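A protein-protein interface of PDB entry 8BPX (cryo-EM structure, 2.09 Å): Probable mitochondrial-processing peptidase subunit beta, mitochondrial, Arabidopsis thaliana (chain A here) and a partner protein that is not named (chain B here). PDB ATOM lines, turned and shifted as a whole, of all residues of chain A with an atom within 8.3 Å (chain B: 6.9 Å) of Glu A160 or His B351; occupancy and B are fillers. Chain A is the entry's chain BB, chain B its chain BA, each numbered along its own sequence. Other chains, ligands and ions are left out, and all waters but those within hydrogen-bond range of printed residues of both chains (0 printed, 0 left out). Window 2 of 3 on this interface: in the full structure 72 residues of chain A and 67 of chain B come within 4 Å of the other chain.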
ATOM      1  N   PHE A 148      -2.953  -7.757  -3.208  1.00  0.00           N
ATOM      2  CA  PHE A 148      -2.950  -6.627  -2.288  1.00  0.00           C
ATOM      3  C   PHE A 148      -2.117  -5.468  -2.828  1.00  0.00           C
ATOM      4  O   PHE A 148      -1.551  -4.692  -2.057  1.00  0.00           O
ATOM      5  CB  PHE A 148      -2.428  -7.049  -0.917  1.00  0.00           C
ATOM      6  CG  PHE A 148      -3.282  -8.068  -0.224  1.00  0.00           C
ATOM      7  CD1 PHE A 148      -4.660  -7.984  -0.262  1.00  0.00           C
ATOM      8  CD2 PHE A 148      -2.700  -9.111   0.475  1.00  0.00           C
ATOM      9  CE1 PHE A 148      -5.436  -8.925   0.376  1.00  0.00           C
ATOM     10  CE2 PHE A 148      -3.476 -10.054   1.114  1.00  0.00           C
ATOM     11  CZ  PHE A 148      -4.845  -9.962   1.064  1.00  0.00           C
ATOM     12  N   LYS A 149      -2.017  -5.342  -4.148  1.00  0.00           N
ATOM     13  CA  LYS A 149      -1.158  -4.340  -4.768  1.00  0.00           C
ATOM     14  C   LYS A 149      -1.947  -3.424  -5.692  1.00  0.00           C
ATOM     15  O   LYS A 149      -1.529  -3.135  -6.815  1.00  0.00           O
ATOM     16  CB  LYS A 149      -0.004  -4.991  -5.523  1.00  0.00           C
ATOM     17  CG  LYS A 149       0.852  -5.905  -4.673  1.00  0.00           C
ATOM     18  CD  LYS A 149       1.453  -5.158  -3.497  1.00  0.00           C
ATOM     19  CE  LYS A 149       2.644  -5.897  -2.932  1.00  0.00           C
ATOM     20  NZ  LYS A 149       3.016  -5.419  -1.569  1.00  0.00           N
ATOM     21  N   ARG A 154      -9.051   1.801  -4.813  1.00  0.00           N
ATOM     22  CA  ARG A 154      -8.091   1.965  -3.676  1.00  0.00           C
ATOM     23  C   ARG A 154      -6.712   1.508  -4.065  1.00  0.00           C
ATOM     24  O   ARG A 154      -6.618   0.501  -4.743  1.00  0.00           O
ATOM     25  CB  ARG A 154      -8.355   1.049  -2.478  1.00  0.00           C
ATOM     26  CG  ARG A 154      -9.800   0.768  -2.124  1.00  0.00           C
ATOM     27  CD  ARG A 154      -9.646  -0.262  -1.034  1.00  0.00           C
ATOM     28  NE  ARG A 154     -10.871  -1.016  -0.891  1.00  0.00           N
ATOM     29  CZ  ARG A 154     -11.830  -0.732  -0.039  1.00  0.00           C
ATOM     30  NH1 ARG A 154     -11.708   0.298   0.774  1.00  0.00           N
ATOM     31  NH2 ARG A 154     -12.902  -1.484   0.005  1.00  0.00           N
ATOM     32  N   THR A 155      -5.685   2.172  -3.576  1.00  0.00           N
ATOM     33  CA  THR A 155      -4.297   1.850  -3.937  1.00  0.00           C
ATOM     34  C   THR A 155      -3.632   1.060  -2.799  1.00  0.00           C
ATOM     35  O   THR A 155      -4.250   0.947  -1.739  1.00  0.00           O
ATOM     36  CB  THR A 155      -3.530   3.155  -4.180  1.00  0.00           C
ATOM     37  OG1 THR A 155      -3.332   3.837  -2.942  1.00  0.00           O
ATOM     38  CG2 THR A 155      -4.209   4.069  -5.179  1.00  0.00           C
ATOM     39  N   VAL A 156      -2.426   0.570  -3.004  1.00  0.00           N
ATOM     40  CA  VAL A 156      -1.674  -0.167  -1.962  1.00  0.00           C
ATOM     41  C   VAL A 156      -1.755   0.602  -0.643  1.00  0.00           C
ATOM     42  O   VAL A 156      -2.158  -0.025   0.348  1.00  0.00           O
ATOM     43  CB  VAL A 156      -0.205  -0.403  -2.358  1.00  0.00           C
ATOM     44  CG1 VAL A 156      -0.095  -1.293  -3.577  1.00  0.00           C
ATOM     45  CG2 VAL A 156       0.538   0.898  -2.576  1.00  0.00           C
ATOM     46  N   ARG A 157      -1.338   1.859  -0.637  1.00  0.00           N
ATOM     47  CA  ARG A 157      -1.361   2.541   0.647  1.00  0.00           C
ATOM     48  C   ARG A 157      -2.779   2.614   1.186  1.00  0.00           C
ATOM     49  O   ARG A 157      -3.049   2.064   2.253  1.00  0.00           O
ATOM     50  CB  ARG A 157      -0.729   3.929   0.534  1.00  0.00           C
ATOM     51  CG  ARG A 157       0.754   3.927   0.885  1.00  0.00           C
ATOM     52  CD  ARG A 157       1.494   5.150   0.364  1.00  0.00           C
ATOM     53  NE  ARG A 157       1.025   5.588  -0.944  1.00  0.00           N
ATOM     54  CZ  ARG A 157       1.378   6.731  -1.518  1.00  0.00           C
ATOM     55  NH1 ARG A 157       2.198   7.580  -0.919  1.00  0.00           N
ATOM     56  NH2 ARG A 157       0.897   7.031  -2.721  1.00  0.00           N
ATOM     57  N   ALA A 158      -3.665   3.185   0.411  1.00  0.00           N
ATOM     58  CA  ALA A 158      -5.072   3.276   0.791  1.00  0.00           C
ATOM     59  C   ALA A 158      -5.587   1.992   1.472  1.00  0.00           C
ATOM     60  O   ALA A 158      -6.243   2.131   2.496  1.00  0.00           O
ATOM     61  CB  ALA A 158      -5.772   3.525  -0.495  1.00  0.00           C
ATOM     62  N   LEU A 159      -5.327   0.813   0.882  1.00  0.00           N
ATOM     63  CA  LEU A 159      -5.736  -0.518   1.400  1.00  0.00           C
ATOM     64  C   LEU A 159      -4.978  -0.884   2.674  1.00  0.00           C
ATOM     65  O   LEU A 159      -5.559  -1.560   3.464  1.00  0.00           O
ATOM     66  CB  LEU A 159      -5.360  -1.544   0.338  1.00  0.00           C
ATOM     67  CG  LEU A 159      -5.930  -2.946   0.523  1.00  0.00           C
ATOM     68  CD1 LEU A 159      -7.231  -3.084  -0.234  1.00  0.00           C
ATOM     69  CD2 LEU A 159      -4.940  -3.991   0.051  1.00  0.00           C
ATOM     70  N   GLU A 160      -3.714  -0.509   2.804  1.00  0.00           N
ATOM     71  CA  GLU A 160      -2.988  -0.765   4.045  1.00  0.00           C
ATOM     72  C   GLU A 160      -3.430   0.135   5.195  1.00  0.00           C
ATOM     73  O   GLU A 160      -3.658  -0.363   6.303  1.00  0.00           O
ATOM     74  CB  GLU A 160      -1.487  -0.600   3.816  1.00  0.00           C
ATOM     75  CG  GLU A 160      -0.850  -1.751   3.069  1.00  0.00           C
ATOM     76  CD  GLU A 160       0.654  -1.780   3.224  1.00  0.00           C
ATOM     77  OE1 GLU A 160       1.282  -0.706   3.124  1.00  0.00           O
ATOM     78  OE2 GLU A 160       1.206  -2.876   3.451  1.00  0.00           O
ATOM     79  N   GLU A 161      -3.564   1.437   4.948  1.00  0.00           N
ATOM     80  CA  GLU A 161      -4.059   2.377   5.944  1.00  0.00           C
ATOM     81  C   GLU A 161      -5.473   2.046   6.392  1.00  0.00           C
ATOM     82  O   GLU A 161      -5.763   2.156   7.579  1.00  0.00           O
ATOM     83  CB  GLU A 161      -4.008   3.821   5.429  1.00  0.00           C
ATOM     84  CG  GLU A 161      -3.016   4.073   4.317  1.00  0.00           C
ATOM     85  CD  GLU A 161      -2.760   5.546   4.059  1.00  0.00           C
ATOM     86  OE1 GLU A 161      -2.119   5.862   3.035  1.00  0.00           O
ATOM     87  OE2 GLU A 161      -3.196   6.385   4.875  1.00  0.00           O
ATOM     88  N   GLU A 162      -6.383   1.624   5.533  1.00  0.00           N
ATOM     89  CA  GLU A 162      -7.735   1.300   6.048  1.00  0.00           C
ATOM     90  C   GLU A 162      -7.743  -0.035   6.818  1.00  0.00           C
ATOM     91  O   GLU A 162      -8.497  -0.198   7.748  1.00  0.00           O
ATOM     92  CB  GLU A 162      -8.775   1.320   4.924  1.00  0.00           C
ATOM     93  CG  GLU A 162      -9.963   0.406   5.069  1.00  0.00           C
ATOM     94  CD  GLU A 162     -10.514  -0.034   3.726  1.00  0.00           C
ATOM     95  OE1 GLU A 162      -9.716  -0.140   2.780  1.00  0.00           O
ATOM     96  OE2 GLU A 162     -11.741  -0.256   3.625  1.00  0.00           O
ATOM     97  N   ILE A 163      -6.937  -0.996   6.441  1.00  0.00           N
ATOM     98  CA  ILE A 163      -6.856  -2.192   7.275  1.00  0.00           C
ATOM     99  C   ILE A 163      -6.280  -1.847   8.643  1.00  0.00           C
ATOM    100  O   ILE A 163      -6.748  -2.347   9.674  1.00  0.00           O
ATOM    101  CB  ILE A 163      -6.041  -3.290   6.568  1.00  0.00           C
ATOM    102  CG1 ILE A 163      -6.769  -3.772   5.312  1.00  0.00           C
ATOM    103  CG2 ILE A 163      -5.785  -4.459   7.507  1.00  0.00           C
ATOM    104  CD1 ILE A 163      -8.254  -3.992   5.502  1.00  0.00           C
ATOM    105  N   GLU A 164      -5.280  -0.966   8.681  1.00  0.00           N
ATOM    106  CA  GLU A 164      -4.691  -0.592   9.963  1.00  0.00           C
ATOM    107  C   GLU A 164      -5.622   0.300  10.777  1.00  0.00           C
ATOM    108  O   GLU A 164      -5.617   0.243  12.013  1.00  0.00           O
ATOM    109  CB  GLU A 164      -3.352   0.099   9.741  1.00  0.00           C
ATOM    110  CG  GLU A 164      -2.293  -0.818   9.196  1.00  0.00           C
ATOM    111  CD  GLU A 164      -1.042  -0.074   8.819  1.00  0.00           C
ATOM    112  OE1 GLU A 164      -1.164   1.035   8.260  1.00  0.00           O
ATOM    113  OE2 GLU A 164       0.060  -0.596   9.083  1.00  0.00           O
ATOM    114  N   ASP A 165      -6.415   1.141  10.109  1.00  0.00           N
ATOM    115  CA  ASP A 165      -7.331   2.022  10.821  1.00  0.00           C
ATOM    116  C   ASP A 165      -8.409   1.227  11.531  1.00  0.00           C
ATOM    117  O   ASP A 165      -8.830   1.595  12.635  1.00  0.00           O
ATOM    118  CB  ASP A 165      -7.966   3.034   9.868  1.00  0.00           C
ATOM    119  CG  ASP A 165      -6.972   4.044   9.336  1.00  0.00           C
ATOM    120  OD1 ASP A 165      -7.286   4.706   8.325  1.00  0.00           O
ATOM    121  OD2 ASP A 165      -5.872   4.163   9.912  1.00  0.00           O
ATOM    122  N   ILE A 166      -8.891   0.146  10.914  1.00  0.00           N
ATOM    123  CA  ILE A 166      -9.789  -0.720  11.677  1.00  0.00           C
ATOM    124  C   ILE A 166      -9.034  -1.674  12.588  1.00  0.00           C
ATOM    125  O   ILE A 166      -9.654  -2.317  13.442  1.00  0.00           O
ATOM    126  CB  ILE A 166     -10.738  -1.536  10.780  1.00  0.00           C
ATOM    127  CG1 ILE A 166      -9.957  -2.377   9.774  1.00  0.00           C
ATOM    128  CG2 ILE A 166     -11.729  -0.616  10.097  1.00  0.00           C
ATOM    129  CD1 ILE A 166     -10.806  -2.915   8.650  1.00  0.00           C
ATOM    130  N   GLY A 167      -7.716  -1.770  12.441  1.00  0.00           N
ATOM    131  CA  GLY A 167      -6.933  -2.693  13.237  1.00  0.00           C
ATOM    132  C   GLY A 167      -7.045  -4.136  12.814  1.00  0.00           C
ATOM    133  O   GLY A 167      -6.762  -5.032  13.614  1.00  0.00           O
ATOM    134  N   GLY A 168      -7.451  -4.392  11.573  1.00  0.00           N
ATOM    135  CA  GLY A 168      -7.675  -5.736  11.093  1.00  0.00           C
ATOM    136  C   GLY A 168      -6.420  -6.392  10.551  1.00  0.00           C
ATOM    137  O   GLY A 168      -5.310  -5.861  10.628  1.00  0.00           O
ATOM    138  N   LEU A 170      -5.145  -8.998   7.115  1.00  0.00           N
ATOM    139  CA  LEU A 170      -5.431  -9.616   5.828  1.00  0.00           C
ATOM    140  C   LEU A 170      -4.398 -10.704   5.582  1.00  0.00           C
ATOM    141  O   LEU A 170      -3.194 -10.430   5.576  1.00  0.00           O
ATOM    142  CB  LEU A 170      -5.412  -8.583   4.700  1.00  0.00           C
ATOM    143  CG  LEU A 170      -6.737  -7.896   4.374  1.00  0.00           C
ATOM    144  CD1 LEU A 170      -6.592  -7.009   3.147  1.00  0.00           C
ATOM    145  CD2 LEU A 170      -7.844  -8.920   4.171  1.00  0.00           C
ATOM    146  N   VAL A 196     -13.626  -4.943   1.060  1.00  0.00           N
ATOM    147  CA  VAL A 196     -12.212  -5.032   0.642  1.00  0.00           C
ATOM    148  C   VAL A 196     -12.007  -6.400  -0.001  1.00  0.00           C
ATOM    149  O   VAL A 196     -11.404  -6.424  -1.051  1.00  0.00           O
ATOM    150  CB  VAL A 196     -11.237  -4.764   1.811  1.00  0.00           C
ATOM    151  CG1 VAL A 196      -9.801  -5.116   1.509  1.00  0.00           C
ATOM    152  CG2 VAL A 196     -11.366  -3.375   2.392  1.00  0.00           C
ATOM    153  N   LEU B 334       3.269   1.480  18.466  1.00  0.00           N
ATOM    154  CA  LEU B 334       3.588   2.639  17.641  1.00  0.00           C
ATOM    155  C   LEU B 334       4.771   2.347  16.728  1.00  0.00           C
ATOM    156  O   LEU B 334       4.745   2.663  15.533  1.00  0.00           O
ATOM    157  CB  LEU B 334       3.881   3.843  18.537  1.00  0.00           C
ATOM    158  CG  LEU B 334       3.517   5.262  18.101  1.00  0.00           C
ATOM    159  CD1 LEU B 334       2.287   5.288  17.207  1.00  0.00           C
ATOM    160  CD2 LEU B 334       3.304   6.131  19.328  1.00  0.00           C
ATOM    161  N   MET B 335       5.824   1.741  17.274  1.00  0.00           N
ATOM    162  CA  MET B 335       6.921   1.272  16.441  1.00  0.00           C
ATOM    163  C   MET B 335       6.619  -0.059  15.769  1.00  0.00           C
ATOM    164  O   MET B 335       7.066  -0.280  14.639  1.00  0.00           O
ATOM    165  CB  MET B 335       8.197   1.145  17.269  1.00  0.00           C
ATOM    166  CG  MET B 335       8.890   2.460  17.511  1.00  0.00           C
ATOM    167  SD  MET B 335       8.552   3.171  19.124  1.00  0.00           S
ATOM    168  CE  MET B 335       9.743   4.497  19.097  1.00  0.00           C
ATOM    169  N   GLY B 345       1.729 -11.382   3.132  1.00  0.00           N
ATOM    170  CA  GLY B 345       0.941 -10.363   2.482  1.00  0.00           C
ATOM    171  C   GLY B 345       0.695  -9.177   3.390  1.00  0.00           C
ATOM    172  O   GLY B 345       0.776  -9.278   4.618  1.00  0.00           O
ATOM    173  N   PRO B 346       0.403  -8.020   2.799  1.00  0.00           N
ATOM    174  CA  PRO B 346       0.107  -6.830   3.605  1.00  0.00           C
ATOM    175  C   PRO B 346      -1.159  -7.018   4.429  1.00  0.00           C
ATOM    176  O   PRO B 346      -1.851  -8.034   4.353  1.00  0.00           O
ATOM    177  CB  PRO B 346      -0.061  -5.721   2.561  1.00  0.00           C
ATOM    178  CG  PRO B 346       0.660  -6.226   1.350  1.00  0.00           C
ATOM    179  CD  PRO B 346       0.471  -7.711   1.362  1.00  0.00           C
ATOM    180  N   GLY B 347      -1.456  -6.005   5.238  1.00  0.00           N
ATOM    181  CA  GLY B 347      -2.575  -6.055   6.153  1.00  0.00           C
ATOM    182  C   GLY B 347      -2.223  -6.499   7.557  1.00  0.00           C
ATOM    183  O   GLY B 347      -3.084  -6.432   8.442  1.00  0.00           O
ATOM    184  N   LYS B 348      -0.990  -6.947   7.786  1.00  0.00           N
ATOM    185  CA  LYS B 348      -0.526  -7.275   9.128  1.00  0.00           C
ATOM    186  C   LYS B 348       0.000  -6.063   9.886  1.00  0.00           C
ATOM    187  O   LYS B 348       0.387  -6.202  11.051  1.00  0.00           O
ATOM    188  CB  LYS B 348       0.562  -8.350   9.065  1.00  0.00           C
ATOM    189  CG  LYS B 348       0.515  -9.223   7.825  1.00  0.00           C
ATOM    190  CD  LYS B 348       0.632 -10.695   8.188  1.00  0.00           C
ATOM    191  CE  LYS B 348       0.476 -11.584   6.964  1.00  0.00           C
ATOM    192  NZ  LYS B 348       0.755 -13.010   7.282  1.00  0.00           N
ATOM    193  N   GLY B 349       0.029  -4.888   9.261  1.00  0.00           N
ATOM    194  CA  GLY B 349       0.471  -3.683   9.934  1.00  0.00           C
ATOM    195  C   GLY B 349       1.909  -3.304   9.644  1.00  0.00           C
ATOM    196  O   GLY B 349       2.669  -2.990  10.566  1.00  0.00           O
ATOM    197  N   MET B 350       2.296  -3.326   8.367  1.00  0.00           N
ATOM    198  CA  MET B 350       3.667  -2.993   7.996  1.00  0.00           C
ATOM    199  C   MET B 350       3.978  -1.509   8.134  1.00  0.00           C
ATOM    200  O   MET B 350       5.158  -1.144   8.155  1.00  0.00           O
ATOM    201  CB  MET B 350       3.953  -3.457   6.564  1.00  0.00           C
ATOM    202  CG  MET B 350       3.860  -2.366   5.509  1.00  0.00           C
ATOM    203  SD  MET B 350       4.334  -2.953   3.871  1.00  0.00           S
ATOM    204  CE  MET B 350       6.090  -3.218   4.099  1.00  0.00           C
ATOM    205  N   HIS B 351       2.963  -0.647   8.238  1.00  0.00           N
ATOM    206  CA  HIS B 351       3.209   0.778   8.432  1.00  0.00           C
ATOM    207  C   HIS B 351       3.635   1.112   9.855  1.00  0.00           C
ATOM    208  O   HIS B 351       3.926   2.281  10.133  1.00  0.00           O
ATOM    209  CB  HIS B 351       1.971   1.595   8.064  1.00  0.00           C
ATOM    210  CG  HIS B 351       1.848   1.881   6.599  1.00  0.00           C
ATOM    211  ND1 HIS B 351       1.680   3.156   6.103  1.00  0.00           N
ATOM    212  CD2 HIS B 351       1.872   1.059   5.524  1.00  0.00           C
ATOM    213  CE1 HIS B 351       1.603   3.106   4.785  1.00  0.00           C
ATOM    214  NE2 HIS B 351       1.718   1.843   4.408  1.00  0.00           N
ATOM    215  N   SER B 352       3.656   0.133  10.760  1.00  0.00           N
ATOM    216  CA  SER B 352       4.224   0.343  12.083  1.00  0.00           C
ATOM    217  C   SER B 352       5.657   0.839  11.950  1.00  0.00           C
ATOM    218  O   SER B 352       6.410   0.372  11.090  1.00  0.00           O
ATOM    219  CB  SER B 352       4.183  -0.958  12.889  1.00  0.00           C
ATOM    220  OG  SER B 352       2.879  -1.223  13.374  1.00  0.00           O
ATOM    221  N   TRP B 353       6.040   1.787  12.805  1.00  0.00           N
ATOM    222  CA  TRP B 353       7.247   2.551  12.514  1.00  0.00           C
ATOM    223  C   TRP B 353       8.514   1.798  12.897  1.00  0.00           C
ATOM    224  O   TRP B 353       9.423   2.368  13.510  1.00  0.00           O
ATOM    225  CB  TRP B 353       7.212   3.893  13.247  1.00  0.00           C
ATOM    226  CG  TRP B 353       6.408   4.949  12.556  1.00  0.00           C
ATOM    227  CD1 TRP B 353       5.280   5.555  13.024  1.00  0.00           C
ATOM    228  CD2 TRP B 353       6.665   5.517  11.267  1.00  0.00           C
ATOM    229  NE1 TRP B 353       4.825   6.473  12.111  1.00  0.00           N
ATOM    230  CE2 TRP B 353       5.654   6.467  11.021  1.00  0.00           C
ATOM    231  CE3 TRP B 353       7.650   5.317  10.297  1.00  0.00           C
ATOM    232  CZ2 TRP B 353       5.603   7.215   9.848  1.00  0.00           C
ATOM    233  CZ3 TRP B 353       7.598   6.061   9.132  1.00  0.00           C
ATOM    234  CH2 TRP B 353       6.582   6.998   8.917  1.00  0.00           C
ATOM    235  N   LEU B 354       8.582   0.528  12.544  1.00  0.00           N
ATOM    236  CA  LEU B 354       9.818  -0.217  12.353  1.00  0.00           C
ATOM    237  C   LEU B 354       9.796  -1.041  11.076  1.00  0.00           C
ATOM    238  O   LEU B 354      10.821  -1.146  10.399  1.00  0.00           O
ATOM    239  CB  LEU B 354      10.101  -1.122  13.560  1.00  0.00           C
ATOM    240  CG  LEU B 354      10.788  -0.434  14.740  1.00  0.00           C
ATOM    241  CD1 LEU B 354      10.557  -1.211  16.024  1.00  0.00           C
ATOM    242  CD2 LEU B 354      12.275  -0.266  14.467  1.00  0.00           C
ATOM    243  N   TYR B 355       8.646  -1.631  10.743  1.00  0.00           N
ATOM    244  CA  TYR B 355       8.548  -2.479   9.525  1.00  0.00           C
ATOM    245  C   TYR B 355       8.742  -1.600   8.284  1.00  0.00           C
ATOM    246  O   TYR B 355       9.544  -1.975   7.410  1.00  0.00           O
ATOM    247  CB  TYR B 355       7.203  -3.210   9.503  1.00  0.00           C
ATOM    248  CG  TYR B 355       7.164  -4.492   8.708  1.00  0.00           C
ATOM    249  CD1 TYR B 355       7.528  -4.527   7.373  1.00  0.00           C
ATOM    250  CD2 TYR B 355       6.731  -5.674   9.287  1.00  0.00           C
ATOM    251  CE1 TYR B 355       7.488  -5.701   6.639  1.00  0.00           C
ATOM    252  CE2 TYR B 355       6.683  -6.857   8.570  1.00  0.00           C
ATOM    253  CZ  TYR B 355       7.062  -6.872   7.241  1.00  0.00           C
ATOM    254  OH  TYR B 355       7.016  -8.034   6.525  1.00  0.00           O
ATOM    255  N   ARG B 356       8.049  -0.460   8.216  1.00  0.00           N
ATOM    256  CA  ARG B 356       8.116   0.423   7.061  1.00  0.00           C
ATOM    257  C   ARG B 356       9.361   1.302   7.078  1.00  0.00           C
ATOM    258  O   ARG B 356       9.577   2.077   6.140  1.00  0.00           O
ATOM    259  CB  ARG B 356       6.853   1.291   6.991  1.00  0.00           C
ATOM    260  CG  ARG B 356       6.606   1.949   5.638  1.00  0.00           C
ATOM    261  CD  ARG B 356       5.315   2.748   5.629  1.00  0.00           C
ATOM    262  NE  ARG B 356       5.158   3.509   4.396  1.00  0.00           N
ATOM    263  CZ  ARG B 356       5.640   4.729   4.203  1.00  0.00           C
ATOM    264  NH1 ARG B 356       6.317   5.363   5.145  1.00  0.00           N
ATOM    265  NH2 ARG B 356       5.437   5.328   3.032  1.00  0.00           N
ATOM    266  N   ARG B 357      10.191   1.195   8.114  1.00  0.00           N
ATOM    267  CA  ARG B 357      11.408   1.986   8.214  1.00  0.00           C
ATOM    268  C   ARG B 357      12.656   1.137   8.015  1.00  0.00           C
ATOM    269  O   ARG B 357      13.433   1.393   7.090  1.00  0.00           O
ATOM    270  CB  ARG B 357      11.460   2.699   9.573  1.00  0.00           C
ATOM    271  CG  ARG B 357      10.737   4.032   9.600  1.00  0.00           C
ATOM    272  CD  ARG B 357      11.597   5.122  10.218  1.00  0.00           C
ATOM    273  NE  ARG B 357      11.000   6.443  10.060  1.00  0.00           N
ATOM    274  CZ  ARG B 357      10.404   7.115  11.036  1.00  0.00           C
ATOM    275  NH1 ARG B 357      10.310   6.621  12.259  1.00  0.00           N
ATOM    276  NH2 ARG B 357       9.890   8.315  10.777  1.00  0.00           N
ATOM    277  N   HIS B 415      -1.054   7.913  12.788  1.00  0.00           N
ATOM    278  CA  HIS B 415      -0.257   6.823  13.333  1.00  0.00           C
ATOM    279  C   HIS B 415      -0.699   6.450  14.743  1.00  0.00           C
ATOM    280  O   HIS B 415      -0.714   5.262  15.087  1.00  0.00           O
ATOM    281  CB  HIS B 415       1.223   7.201  13.303  1.00  0.00           C
ATOM    282  CG  HIS B 415       1.737   7.493  11.928  1.00  0.00           C
ATOM    283  ND1 HIS B 415       1.957   8.775  11.473  1.00  0.00           N
ATOM    284  CD2 HIS B 415       2.053   6.671  10.900  1.00  0.00           C
ATOM    285  CE1 HIS B 415       2.401   8.729  10.229  1.00  0.00           C
ATOM    286  NE2 HIS B 415       2.466   7.464   9.858  1.00  0.00           N
ATOM    287  N   ARG B 418      -3.845   4.429  14.443  1.00  0.00           N
ATOM    288  CA  ARG B 418      -3.514   3.091  13.964  1.00  0.00           C
ATOM    289  C   ARG B 418      -2.944   2.231  15.089  1.00  0.00           C
ATOM    290  O   ARG B 418      -3.319   1.063  15.247  1.00  0.00           O
ATOM    291  CB  ARG B 418      -2.539   3.176  12.787  1.00  0.00           C
ATOM    292  CG  ARG B 418      -3.196   3.626  11.488  1.00  0.00           C
ATOM    293  CD  ARG B 418      -2.182   3.834  10.370  1.00  0.00           C
ATOM    294  NE  ARG B 418      -2.532   4.964   9.517  1.00  0.00           N
ATOM    295  CZ  ARG B 418      -1.766   5.432   8.542  1.00  0.00           C
ATOM    296  NH1 ARG B 418      -0.587   4.893   8.267  1.00  0.00           N
ATOM    297  NH2 ARG B 418      -2.190   6.466   7.822  1.00  0.00           N
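Hydrophobic or aromatic side chains of chain B within 4 Å of the printed part of chain A: Pro B346, Met B350 and His B351.
Hydrophobic or aromatic side chains of chain A that line the printed part of chain B: Phe A148, Ile A163 and Leu A170.
Among the printed residues, Asp or Glu carboxylates within 4 Å of a Lys or Arg side-chain nitrogen of the other chain: Glu A161 with Arg B418, Glu A164 with Arg B418 and Asp A165 with Arg B418.
A ring nitrogen (NE2) of His B351 lies within hydrogen-bond range of the side-chain carboxylate (OE1) of Glu A160, 2.9 Å away.
The side-chain carboxylate of Glu A164 sits at hydrogen-bond distance from the backbone NH of His B351 (3.0 Å).
The guanidinium group of Arg B418 lies within salt-bridge range of the side-chain carboxylate of Glu A161 (3.1 Å).
The guanidinium group (NH1) of Arg B418 lies within salt-bridge range of the side-chain carboxylate (OE1) of Glu A164 (3.9 Å).
The guanidinium group of Arg B418 lies within salt-bridge range of the side-chain carboxylate of Asp A165.
The side-chain sulfur (SD) of Met B350 sits close to the side-chain carboxylate (OE2) of Glu A160, 3.2 Å away.
O of Gly A168 sits close to O of Gly B347 (3.2 Å).
The backbone carbonyl oxygen of Pro B346 lies close to the backbone carbonyl oxygen of Leu A170 (3.0 Å).
Among the printed residues, pairs that only touch across the chains: Phe A148 with Pro B346 (3.6 Å), Lys A149 with Pro B346 (3.8 Å), Glu A160 with Pro B346 (3.2 Å), Ile A163 with Gly B347 (3.5 Å), Glu A164 with Gly B349 (3.2 Å), Glu A164 with Met B350 (3.6 Å) and Leu A170 with Gly B347 (3.5 Å).
Printed residues of chain B within 4 Å of Phe A148: Pro B346.
Printed residues of chain B within 4 Å of Lys A149: Pro B346 (3.8 Å).
Of chain B, only Pro B346 (3.2 Å), Met B350 (3.2 Å) and His B351 (2.9 Å) come within 4 Å of Glu A160.
Printed residues of chain A within 4 Å of Gly B347: Ile A163, Gly A168 and Leu A170.
Of the printed residues of chain A, Met B350 touches Glu A160 and Glu A164.
Of chain A, only Glu A160 and Glu A164 come within 4 Å of His B351.
Of the printed residues of chain A, Arg B418 touches Glu A161 (3.1 Å), Glu A164 (3.7 Å) and Asp A165 (3.2 Å).
The nearest residue of chain B that does not touch Glu A160 is Gly B347 (4.5 Å).
The nearest residue of chain A that does not touch His B351 is Arg A157 (4.1 Å).
The nearest printed residue of chain A that does not touch Arg B418 is Gly A167 (5.6 Å).
The backbone carbonyl oxygen (O) of Gly B349 lies within hydrogen-bond range of the side-chain hydroxyl (OG) of Ser B352 (3.3 Å).
O of Met B350 sits at hydrogen-bond distance from N of Arg B356 (3.0 Å).
N of Gly A168 is in hydrogen-bond range of O of Ile A163 (2.9 Å).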
